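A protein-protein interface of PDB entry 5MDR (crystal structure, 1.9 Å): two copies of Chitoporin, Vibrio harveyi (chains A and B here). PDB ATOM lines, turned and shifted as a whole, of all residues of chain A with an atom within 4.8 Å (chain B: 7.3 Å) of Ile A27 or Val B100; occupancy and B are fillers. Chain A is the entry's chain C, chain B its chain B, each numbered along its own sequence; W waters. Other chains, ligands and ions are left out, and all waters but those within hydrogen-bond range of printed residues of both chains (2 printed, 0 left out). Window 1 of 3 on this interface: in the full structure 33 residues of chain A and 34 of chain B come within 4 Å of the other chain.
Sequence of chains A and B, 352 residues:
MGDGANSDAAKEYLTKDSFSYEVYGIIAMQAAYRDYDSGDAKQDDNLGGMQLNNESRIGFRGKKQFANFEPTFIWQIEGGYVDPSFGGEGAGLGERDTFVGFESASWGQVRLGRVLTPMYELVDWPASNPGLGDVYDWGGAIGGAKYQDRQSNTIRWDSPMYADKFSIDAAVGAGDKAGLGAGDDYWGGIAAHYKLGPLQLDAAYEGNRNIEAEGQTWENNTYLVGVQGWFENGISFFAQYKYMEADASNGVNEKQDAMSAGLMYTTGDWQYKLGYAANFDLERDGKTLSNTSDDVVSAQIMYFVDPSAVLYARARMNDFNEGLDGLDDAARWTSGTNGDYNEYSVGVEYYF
The backbone NH of Gly B113 sits at hydrogen-bond distance from the backbone carbonyl oxygen of Thr B154 (2.9 Å).
O of Phe B60 is in hydrogen-bond range of N of Ile B77 (2.8 Å).
The backbone carbonyl oxygen (O) of Tyr A350 is in hydrogen-bond range of the backbone NH (N) of Ile A27.
The backbone NH (N) of Gly A25 is in hydrogen-bond range of the chain-end carboxylate (OXT) of Phe A352 (3.0 Å).
The backbone NH (N) of Ala A28 is in hydrogen-bond range of the side-chain hydroxyl (OG) of Ser A56.
O of Met A29 sits at hydrogen-bond distance from N of Val A348 (2.9 Å).
Among the printed residues, merely in contact across the chains: Met A29 with Leu B112 (3.3 Å), Ile A27 with Val B100 (3.5 Å), Met A29 with Val B100 (3.6 Å), Phe A352 with Trp B75 (3.6 Å), Ile A27 with Trp B75 (3.7 Å), Tyr A350 with Trp B75 (3.7 Å), Ile A27 with Phe B73 (3.9 Å), Tyr A350 with Phe B73 (3.9 Å), Met A29 with Gly B113 (3.9 Å), Ile A27 with Ile B77 (3.97 Å) and Ser A56 with Ile B77 (3.98 Å).
Ile A27 touches four residues of chain B.
Of the printed residues of chain B, Tyr A350 touches Phe B73 (3.9 Å) and Trp B75 (3.7 Å).
Of the printed residues of chain A, Trp B75 touches Ile A27, Tyr A350 and Phe A352.
Val B100 touches just these residues of chain A: Ile A27 and Met A29.
Printed residues of chain A within 4 Å of Leu B112: Met A29.
Arg B114 touches none of the printed residues of chain A.
The nearest residue of chain A that does not touch Val B100 is Val A348 (4.3 Å).
Hydrophobic or aromatic side chains of chain A within 4 Å of the printed part of chain B: Ile A27, Met A29, Tyr A350 and Phe A352.
Of the 19 printed residues of chain B, 6 touch a printed residue of chain A.
Printed residues of chain B that touch a printed residue of chain A: Phe B73, Trp B75, Ile B77, Val B100, Leu B112 and Gly B113.
Hydrophobic or aromatic side chains of chain B that line the printed part of chain A: Phe B73, Trp B75, Ile B77 and Val B100.
No position is printed for both chains.
Of the 11 pairs that touch across the chains among the printed residues, none has its exchanged pair printed and touching as well.
Water W2 bridges the side-chain hydroxyl (OH) of Tyr A350 and the indole nitrogen (NE1) of Trp B75.
Water W1 lies within hydrogen-bond range of the backbone carbonyl oxygen of Phe B99, the side-chain hydroxyl of Ser A56 and the backbone carbonyl oxygen of Gln B76.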
ATOM      1  N   GLY A  25      22.441 -27.057 -21.830  1.00  0.00           N
ATOM      2  CA  GLY A  25      21.870 -25.817 -21.360  1.00  0.00           C
ATOM      3  C   GLY A  25      22.451 -25.304 -20.081  1.00  0.00           C
ATOM      4  O   GLY A  25      23.069 -26.050 -19.316  1.00  0.00           O
ATOM      5  N   ILE A  26      22.278 -23.999 -19.897  1.00  0.00           N
ATOM      6  CA  ILE A  26      22.559 -23.357 -18.642  1.00  0.00           C
ATOM      7  C   ILE A  26      21.275 -22.657 -18.259  1.00  0.00           C
ATOM      8  O   ILE A  26      20.802 -21.782 -18.983  1.00  0.00           O
ATOM      9  CB  ILE A  26      23.719 -22.339 -18.735  1.00  0.00           C
ATOM     10  CG1 ILE A  26      25.038 -23.064 -19.115  1.00  0.00           C
ATOM     11  CG2 ILE A  26      23.903 -21.664 -17.375  1.00  0.00           C
ATOM     12  CD1 ILE A  26      25.229 -23.235 -20.613  1.00  0.00           C
ATOM     13  N   ILE A  27      20.693 -23.090 -17.155  1.00  0.00           N
ATOM     14  CA  ILE A  27      19.442 -22.507 -16.668  1.00  0.00           C
ATOM     15  C   ILE A  27      19.847 -21.566 -15.557  1.00  0.00           C
ATOM     16  O   ILE A  27      20.425 -22.013 -14.552  1.00  0.00           O
ATOM     17  CB  ILE A  27      18.495 -23.589 -16.159  1.00  0.00           C
ATOM     18  CG1 ILE A  27      18.211 -24.658 -17.245  1.00  0.00           C
ATOM     19  CG2 ILE A  27      17.181 -22.976 -15.644  1.00  0.00           C
ATOM     20  CD1 ILE A  27      17.754 -24.085 -18.574  1.00  0.00           C
ATOM     21  N   ALA A  28      19.607 -20.275 -15.749  1.00  0.00           N
ATOM     22  CA  ALA A  28      20.155 -19.258 -14.871  1.00  0.00           C
ATOM     23  C   ALA A  28      19.130 -18.179 -14.657  1.00  0.00           C
ATOM     24  O   ALA A  28      18.681 -17.541 -15.635  1.00  0.00           O
ATOM     25  CB  ALA A  28      21.403 -18.634 -15.482  1.00  0.00           C
ATOM     26  N   MET A  29      18.759 -17.964 -13.390  1.00  0.00           N
ATOM     27  CA  MET A  29      17.742 -16.960 -13.034  1.00  0.00           C
ATOM     28  C   MET A  29      18.261 -16.189 -11.857  1.00  0.00           C
ATOM     29  O   MET A  29      18.649 -16.785 -10.832  1.00  0.00           O
ATOM     30  CB  MET A  29      16.414 -17.613 -12.668  1.00  0.00           C
ATOM     31  CG  MET A  29      15.350 -16.641 -12.116  1.00  0.00           C
ATOM     32  SD  MET A  29      14.821 -15.368 -13.488  1.00  0.00           S
ATOM     33  CE  MET A  29      13.809 -16.627 -14.550  1.00  0.00           C
ATOM     34  N   SER A  56      19.098 -17.904 -18.890  1.00  0.00           N
ATOM     35  CA  SER A  56      19.050 -19.261 -19.388  1.00  0.00           C
ATOM     36  C   SER A  56      19.325 -19.271 -20.909  1.00  0.00           C
ATOM     37  O   SER A  56      18.955 -18.331 -21.640  1.00  0.00           O
ATOM     38  CB  SER A  56      17.705 -19.933 -19.074  1.00  0.00           C
ATOM     39  OG  SER A  56      17.395 -19.934 -17.707  1.00  0.00           O
ATOM     40  N   VAL A 348      19.947 -18.681  -9.087  1.00  0.00           N
ATOM     41  CA  VAL A 348      20.167 -20.103  -9.261  1.00  0.00           C
ATOM     42  C   VAL A 348      20.819 -20.289 -10.609  1.00  0.00           C
ATOM     43  O   VAL A 348      20.446 -19.609 -11.583  1.00  0.00           O
ATOM     44  CB  VAL A 348      18.851 -20.932  -9.131  1.00  0.00           C
ATOM     45  CG1 VAL A 348      17.766 -20.461 -10.121  1.00  0.00           C
ATOM     46  CG2 VAL A 348      19.122 -22.427  -9.317  1.00  0.00           C
ATOM     47  N   GLU A 349      21.799 -21.187 -10.693  1.00  0.00           N
ATOM     48  CA  GLU A 349      22.328 -21.623 -11.992  1.00  0.00           C
ATOM     49  C   GLU A 349      22.462 -23.138 -11.985  1.00  0.00           C
ATOM     50  O   GLU A 349      22.957 -23.717 -11.014  1.00  0.00           O
ATOM     51  CB  GLU A 349      23.684 -20.987 -12.332  1.00  0.00           C
ATOM     52  CG  GLU A 349      23.636 -19.481 -12.310  1.00  0.00           C
ATOM     53  CD  GLU A 349      24.707 -18.786 -13.156  1.00  0.00           C
ATOM     54  OE1 GLU A 349      25.679 -19.471 -13.601  1.00  0.00           O
ATOM     55  OE2 GLU A 349      24.545 -17.532 -13.348  1.00  0.00           O
ATOM     56  N   TYR A 350      22.010 -23.757 -13.070  1.00  0.00           N
ATOM     57  CA  TYR A 350      21.972 -25.217 -13.218  1.00  0.00           C
ATOM     58  C   TYR A 350      22.470 -25.543 -14.633  1.00  0.00           C
ATOM     59  O   TYR A 350      22.043 -24.903 -15.591  1.00  0.00           O
ATOM     60  CB  TYR A 350      20.546 -25.737 -12.985  1.00  0.00           C
ATOM     61  CG  TYR A 350      20.215 -27.115 -13.532  1.00  0.00           C
ATOM     62  CD1 TYR A 350      20.849 -28.257 -13.054  1.00  0.00           C
ATOM     63  CD2 TYR A 350      19.262 -27.275 -14.530  1.00  0.00           C
ATOM     64  CE1 TYR A 350      20.520 -29.519 -13.525  1.00  0.00           C
ATOM     65  CE2 TYR A 350      18.934 -28.523 -15.016  1.00  0.00           C
ATOM     66  CZ  TYR A 350      19.564 -29.648 -14.512  1.00  0.00           C
ATOM     67  OH  TYR A 350      19.223 -30.901 -14.994  1.00  0.00           O
ATOM     68  N   PHE A 352      23.263 -28.548 -17.602  1.00  0.00           N
ATOM     69  CA  PHE A 352      23.099 -29.907 -18.105  1.00  0.00           C
ATOM     70  C   PHE A 352      23.646 -30.029 -19.528  1.00  0.00           C
ATOM     71  O   PHE A 352      23.730 -31.172 -19.976  1.00  0.00           O
ATOM     72  CB  PHE A 352      21.626 -30.345 -18.064  1.00  0.00           C
ATOM     73  CG  PHE A 352      20.737 -29.616 -19.036  1.00  0.00           C
ATOM     74  CD1 PHE A 352      20.578 -30.089 -20.334  1.00  0.00           C
ATOM     75  CD2 PHE A 352      20.080 -28.468 -18.664  1.00  0.00           C
ATOM     76  CE1 PHE A 352      19.772 -29.431 -21.240  1.00  0.00           C
ATOM     77  CE2 PHE A 352      19.287 -27.792 -19.570  1.00  0.00           C
ATOM     78  CZ  PHE A 352      19.132 -28.267 -20.866  1.00  0.00           C
ATOM     79  OXT PHE A 352      23.964 -29.056 -20.220  1.00  0.00           O
ATOM     80  N   PHE B  60      11.509 -26.476 -24.628  1.00  0.00           N
ATOM     81  CA  PHE B  60      12.394 -27.343 -23.859  1.00  0.00           C
ATOM     82  C   PHE B  60      11.956 -27.210 -22.405  1.00  0.00           C
ATOM     83  O   PHE B  60      11.664 -26.107 -21.929  1.00  0.00           O
ATOM     84  CB  PHE B  60      13.849 -26.893 -23.951  1.00  0.00           C
ATOM     85  CG  PHE B  60      14.388 -26.915 -25.342  1.00  0.00           C
ATOM     86  CD1 PHE B  60      14.121 -25.886 -26.210  1.00  0.00           C
ATOM     87  CD2 PHE B  60      15.182 -27.974 -25.779  1.00  0.00           C
ATOM     88  CE1 PHE B  60      14.624 -25.910 -27.524  1.00  0.00           C
ATOM     89  CE2 PHE B  60      15.674 -28.011 -27.083  1.00  0.00           C
ATOM     90  CZ  PHE B  60      15.378 -26.976 -27.954  1.00  0.00           C
ATOM     91  N   PHE B  73      13.452 -28.804  -8.490  1.00  0.00           N
ATOM     92  CA  PHE B  73      13.689 -27.694  -9.430  1.00  0.00           C
ATOM     93  C   PHE B  73      13.004 -27.982 -10.752  1.00  0.00           C
ATOM     94  O   PHE B  73      13.093 -29.085 -11.283  1.00  0.00           O
ATOM     95  CB  PHE B  73      15.192 -27.515  -9.666  1.00  0.00           C
ATOM     96  CG  PHE B  73      15.549 -26.312 -10.517  1.00  0.00           C
ATOM     97  CD1 PHE B  73      15.330 -25.040 -10.063  1.00  0.00           C
ATOM     98  CD2 PHE B  73      16.175 -26.482 -11.751  1.00  0.00           C
ATOM     99  CE1 PHE B  73      15.689 -23.923 -10.824  1.00  0.00           C
ATOM    100  CE2 PHE B  73      16.549 -25.375 -12.538  1.00  0.00           C
ATOM    101  CZ  PHE B  73      16.318 -24.090 -12.058  1.00  0.00           C
ATOM    102  N   ILE B  74      12.345 -26.973 -11.304  1.00  0.00           N
ATOM    103  CA  ILE B  74      11.694 -27.074 -12.611  1.00  0.00           C
ATOM    104  C   ILE B  74      12.100 -25.908 -13.495  1.00  0.00           C
ATOM    105  O   ILE B  74      12.411 -24.811 -13.014  1.00  0.00           O
ATOM    106  CB  ILE B  74      10.149 -27.140 -12.509  1.00  0.00           C
ATOM    107  CG1 ILE B  74       9.562 -25.847 -11.941  1.00  0.00           C
ATOM    108  CG2 ILE B  74       9.730 -28.323 -11.634  1.00  0.00           C
ATOM    109  CD1 ILE B  74       8.019 -25.819 -11.876  1.00  0.00           C
ATOM    110  N   TRP B  75      12.074 -26.139 -14.807  1.00  0.00           N
ATOM    111  CA  TRP B  75      12.369 -25.081 -15.753  1.00  0.00           C
ATOM    112  C   TRP B  75      11.700 -25.366 -17.099  1.00  0.00           C
ATOM    113  O   TRP B  75      11.397 -26.516 -17.445  1.00  0.00           O
ATOM    114  CB  TRP B  75      13.897 -24.895 -15.923  1.00  0.00           C
ATOM    115  CG  TRP B  75      14.573 -26.115 -16.487  1.00  0.00           C
ATOM    116  CD1 TRP B  75      15.073 -27.182 -15.775  1.00  0.00           C
ATOM    117  CD2 TRP B  75      14.786 -26.418 -17.863  1.00  0.00           C
ATOM    118  NE1 TRP B  75      15.590 -28.121 -16.633  1.00  0.00           N
ATOM    119  CE2 TRP B  75      15.423 -27.683 -17.919  1.00  0.00           C
ATOM    120  CE3 TRP B  75      14.493 -25.748 -19.055  1.00  0.00           C
ATOM    121  CZ2 TRP B  75      15.770 -28.294 -19.121  1.00  0.00           C
ATOM    122  CZ3 TRP B  75      14.843 -26.351 -20.256  1.00  0.00           C
ATOM    123  CH2 TRP B  75      15.487 -27.605 -20.274  1.00  0.00           C
ATOM    124  N   GLN B  76      11.523 -24.293 -17.855  1.00  0.00           N
ATOM    125  CA  GLN B  76      10.948 -24.360 -19.191  1.00  0.00           C
ATOM    126  C   GLN B  76      11.421 -23.174 -19.999  1.00  0.00           C
ATOM    127  O   GLN B  76      11.527 -22.064 -19.481  1.00  0.00           O
ATOM    128  CB  GLN B  76       9.404 -24.356 -19.119  1.00  0.00           C
ATOM    129  CG  GLN B  76       8.697 -24.345 -20.459  1.00  0.00           C
ATOM    130  CD  GLN B  76       7.196 -24.466 -20.292  1.00  0.00           C
ATOM    131  OE1 GLN B  76       6.734 -25.500 -19.853  1.00  0.00           O
ATOM    132  NE2 GLN B  76       6.437 -23.415 -20.624  1.00  0.00           N
ATOM    133  N   ILE B  77      11.668 -23.423 -21.281  1.00  0.00           N
ATOM    134  CA  ILE B  77      11.967 -22.375 -22.234  1.00  0.00           C
ATOM    135  C   ILE B  77      11.134 -22.658 -23.486  1.00  0.00           C
ATOM    136  O   ILE B  77      11.397 -23.629 -24.192  1.00  0.00           O
ATOM    137  CB  ILE B  77      13.473 -22.368 -22.602  1.00  0.00           C
ATOM    138  CG1 ILE B  77      14.357 -22.128 -21.367  1.00  0.00           C
ATOM    139  CG2 ILE B  77      13.738 -21.322 -23.703  1.00  0.00           C
ATOM    140  CD1 ILE B  77      15.830 -22.377 -21.601  1.00  0.00           C
ATOM    141  N   THR B  98       8.345 -19.185 -19.974  1.00  0.00           N
ATOM    142  CA  THR B  98       9.775 -19.419 -19.852  1.00  0.00           C
ATOM    143  C   THR B  98      10.143 -19.026 -18.421  1.00  0.00           C
ATOM    144  O   THR B  98      10.014 -17.866 -18.043  1.00  0.00           O
ATOM    145  CB  THR B  98      10.537 -18.570 -20.909  1.00  0.00           C
ATOM    146  OG1 THR B  98      10.213 -19.061 -22.231  1.00  0.00           O
ATOM    147  CG2 THR B  98      12.037 -18.624 -20.727  1.00  0.00           C
ATOM    148  N   PHE B  99      10.575 -20.010 -17.653  1.00  0.00           N
ATOM    149  CA  PHE B  99      10.693 -19.826 -16.211  1.00  0.00           C
ATOM    150  C   PHE B  99      11.594 -20.838 -15.564  1.00  0.00           C
ATOM    151  O   PHE B  99      11.988 -21.818 -16.186  1.00  0.00           O
ATOM    152  CB  PHE B  99       9.261 -19.896 -15.559  1.00  0.00           C
ATOM    153  CG  PHE B  99       8.518 -21.159 -15.839  1.00  0.00           C
ATOM    154  CD1 PHE B  99       8.797 -22.324 -15.139  1.00  0.00           C
ATOM    155  CD2 PHE B  99       7.539 -21.209 -16.835  1.00  0.00           C
ATOM    156  CE1 PHE B  99       8.105 -23.509 -15.409  1.00  0.00           C
ATOM    157  CE2 PHE B  99       6.832 -22.384 -17.089  1.00  0.00           C
ATOM    158  CZ  PHE B  99       7.123 -23.543 -16.382  1.00  0.00           C
ATOM    159  N   VAL B 100      11.884 -20.595 -14.272  1.00  0.00           N
ATOM    160  CA  VAL B 100      12.450 -21.590 -13.395  1.00  0.00           C
ATOM    161  C   VAL B 100      11.508 -21.665 -12.217  1.00  0.00           C
ATOM    162  O   VAL B 100      10.649 -20.779 -12.032  1.00  0.00           O
ATOM    163  CB  VAL B 100      13.883 -21.240 -12.902  1.00  0.00           C
ATOM    164  CG1 VAL B 100      14.783 -20.991 -14.091  1.00  0.00           C
ATOM    165  CG2 VAL B 100      13.875 -20.022 -11.980  1.00  0.00           C
ATOM    166  N   GLY B 101      11.651 -22.684 -11.408  1.00  0.00           N
ATOM    167  CA  GLY B 101      10.798 -22.772 -10.223  1.00  0.00           C
ATOM    168  C   GLY B 101      11.105 -23.939  -9.340  1.00  0.00           C
ATOM    169  O   GLY B 101      12.074 -24.683  -9.575  1.00  0.00           O
ATOM    170  N   PHE B 102      10.265 -24.109  -8.326  1.00  0.00           N
ATOM    171  CA  PHE B 102      10.339 -25.225  -7.427  1.00  0.00           C
ATOM    172  C   PHE B 102       8.941 -25.734  -7.145  1.00  0.00           C
ATOM    173  O   PHE B 102       7.981 -24.973  -7.184  1.00  0.00           O
ATOM    174  CB  PHE B 102      11.003 -24.840  -6.105  1.00  0.00           C
ATOM    175  CG  PHE B 102      12.446 -24.482  -6.236  1.00  0.00           C
ATOM    176  CD1 PHE B 102      13.424 -25.464  -6.232  1.00  0.00           C
ATOM    177  CD2 PHE B 102      12.825 -23.158  -6.399  1.00  0.00           C
ATOM    178  CE1 PHE B 102      14.761 -25.139  -6.355  1.00  0.00           C
ATOM    179  CE2 PHE B 102      14.172 -22.830  -6.562  1.00  0.00           C
ATOM    180  CZ  PHE B 102      15.128 -23.813  -6.518  1.00  0.00           C
ATOM    181  N   VAL B 110       6.049 -22.784  -7.346  1.00  0.00           N
ATOM    182  CA  VAL B 110       6.370 -21.383  -7.513  1.00  0.00           C
ATOM    183  C   VAL B 110       7.236 -21.288  -8.748  1.00  0.00           C
ATOM    184  O   VAL B 110       8.177 -22.068  -8.916  1.00  0.00           O
ATOM    185  CB  VAL B 110       7.027 -20.774  -6.258  1.00  0.00           C
ATOM    186  CG1 VAL B 110       8.322 -21.494  -5.904  1.00  0.00           C
ATOM    187  CG2 VAL B 110       7.318 -19.287  -6.445  1.00  0.00           C
ATOM    188  N   ARG B 111       6.900 -20.326  -9.604  1.00  0.00           N
ATOM    189  CA  ARG B 111       7.645 -20.044 -10.809  1.00  0.00           C
ATOM    190  C   ARG B 111       8.101 -18.592 -10.848  1.00  0.00           C
ATOM    191  O   ARG B 111       7.395 -17.692 -10.381  1.00  0.00           O
ATOM    192  CB  ARG B 111       6.791 -20.355 -12.034  1.00  0.00           C
ATOM    193  CG  ARG B 111       6.533 -21.850 -12.207  1.00  0.00           C
ATOM    194  CD  ARG B 111       5.630 -22.072 -13.408  1.00  0.00           C
ATOM    195  NE  ARG B 111       4.245 -21.646 -13.154  1.00  0.00           N
ATOM    196  CZ  ARG B 111       3.337 -21.335 -14.096  1.00  0.00           C
ATOM    197  NH1 ARG B 111       3.639 -21.362 -15.395  1.00  0.00           N
ATOM    198  NH2 ARG B 111       2.111 -20.971 -13.741  1.00  0.00           N
ATOM    199  N   LEU B 112       9.306 -18.387 -11.367  1.00  0.00           N
ATOM    200  CA  LEU B 112       9.867 -17.075 -11.608  1.00  0.00           C
ATOM    201  C   LEU B 112      10.197 -16.981 -13.093  1.00  0.00           C
ATOM    202  O   LEU B 112      10.868 -17.873 -13.640  1.00  0.00           O
ATOM    203  CB  LEU B 112      11.153 -16.876 -10.839  1.00  0.00           C
ATOM    204  CG  LEU B 112      11.055 -16.635  -9.323  1.00  0.00           C
ATOM    205  CD1 LEU B 112      10.542 -17.863  -8.665  1.00  0.00           C
ATOM    206  CD2 LEU B 112      12.469 -16.384  -8.778  1.00  0.00           C
ATOM    207  N   GLY B 113       9.766 -15.901 -13.710  1.00  0.00           N
ATOM    208  CA  GLY B 113      10.112 -15.624 -15.108  1.00  0.00           C
ATOM    209  C   GLY B 113       8.946 -15.056 -15.875  1.00  0.00           C
ATOM    210  O   GLY B 113       8.344 -14.062 -15.459  1.00  0.00           O
ATOM    211  N   ARG B 114       8.630 -15.718 -16.972  1.00  0.00           N
ATOM    212  CA  ARG B 114       7.623 -15.266 -17.924  1.00  0.00           C
ATOM    213  C   ARG B 114       6.493 -16.286 -17.943  1.00  0.00           C
ATOM    214  O   ARG B 114       6.668 -17.422 -18.400  1.00  0.00           O
ATOM    215  CB  ARG B 114       8.262 -15.117 -19.329  1.00  0.00           C
ATOM    216  CG  ARG B 114       7.294 -14.618 -20.414  1.00  0.00           C
ATOM    217  CD  ARG B 114       8.051 -14.362 -21.716  1.00  0.00           C
ATOM    218  NE  ARG B 114       7.150 -13.901 -22.749  1.00  0.00           N
ATOM    219  CZ  ARG B 114       6.585 -12.678 -22.786  1.00  0.00           C
ATOM    220  NH1 ARG B 114       6.884 -11.717 -21.913  1.00  0.00           N
ATOM    221  NH2 ARG B 114       5.714 -12.412 -23.749  1.00  0.00           N
ATOM    222  N   VAL B 115       5.340 -15.868 -17.416  1.00  0.00           N
ATOM    223  CA  VAL B 115       4.175 -16.754 -17.237  1.00  0.00           C
ATOM    224  C   VAL B 115       2.908 -15.942 -17.474  1.00  0.00           C
ATOM    225  O   VAL B 115       2.940 -14.696 -17.595  1.00  0.00           O
ATOM    226  CB  VAL B 115       4.133 -17.385 -15.825  1.00  0.00           C
ATOM    227  CG1 VAL B 115       5.365 -18.223 -15.555  1.00  0.00           C
ATOM    228  CG2 VAL B 115       4.004 -16.324 -14.739  1.00  0.00           C
ATOM    229  N   THR B 154       7.989 -11.928 -13.430  1.00  0.00           N
ATOM    230  CA  THR B 154       6.839 -12.337 -12.626  1.00  0.00           C
ATOM    231  C   THR B 154       7.236 -13.469 -11.665  1.00  0.00           C
ATOM    232  O   THR B 154       8.011 -14.354 -12.019  1.00  0.00           O
ATOM    233  CB  THR B 154       5.710 -12.847 -13.549  1.00  0.00           C
ATOM    234  OG1 THR B 154       5.316 -11.779 -14.409  1.00  0.00           O
ATOM    235  CG2 THR B 154       4.510 -13.317 -12.766  1.00  0.00           C
ATOM    236  N   ARG B 156       4.986 -16.331  -9.589  1.00  0.00           N
ATOM    237  CA  ARG B 156       3.651 -16.881  -9.529  1.00  0.00           C
ATOM    238  C   ARG B 156       3.637 -18.159  -8.707  1.00  0.00           C
ATOM    239  O   ARG B 156       4.448 -19.063  -8.947  1.00  0.00           O
ATOM    240  CB  ARG B 156       3.092 -17.144 -10.941  1.00  0.00           C
ATOM    241  CG  ARG B 156       1.750 -17.856 -10.917  1.00  0.00           C
ATOM    242  CD  ARG B 156       1.025 -17.878 -12.256  1.00  0.00           C
ATOM    243  NE  ARG B 156       0.021 -18.949 -12.245  1.00  0.00           N
ATOM    244  CZ  ARG B 156      -0.938 -19.116 -13.162  1.00  0.00           C
ATOM    245  NH1 ARG B 156      -1.099 -18.252 -14.166  1.00  0.00           N
ATOM    246  NH2 ARG B 156      -1.734 -20.161 -13.091  1.00  0.00           N
HETATM  247  O   HOH W   1      14.119 -20.313 -18.103  1.00  0.00           O
HETATM  248  O   HOH W   2      16.756 -30.813 -15.979  1.00  0.00           O
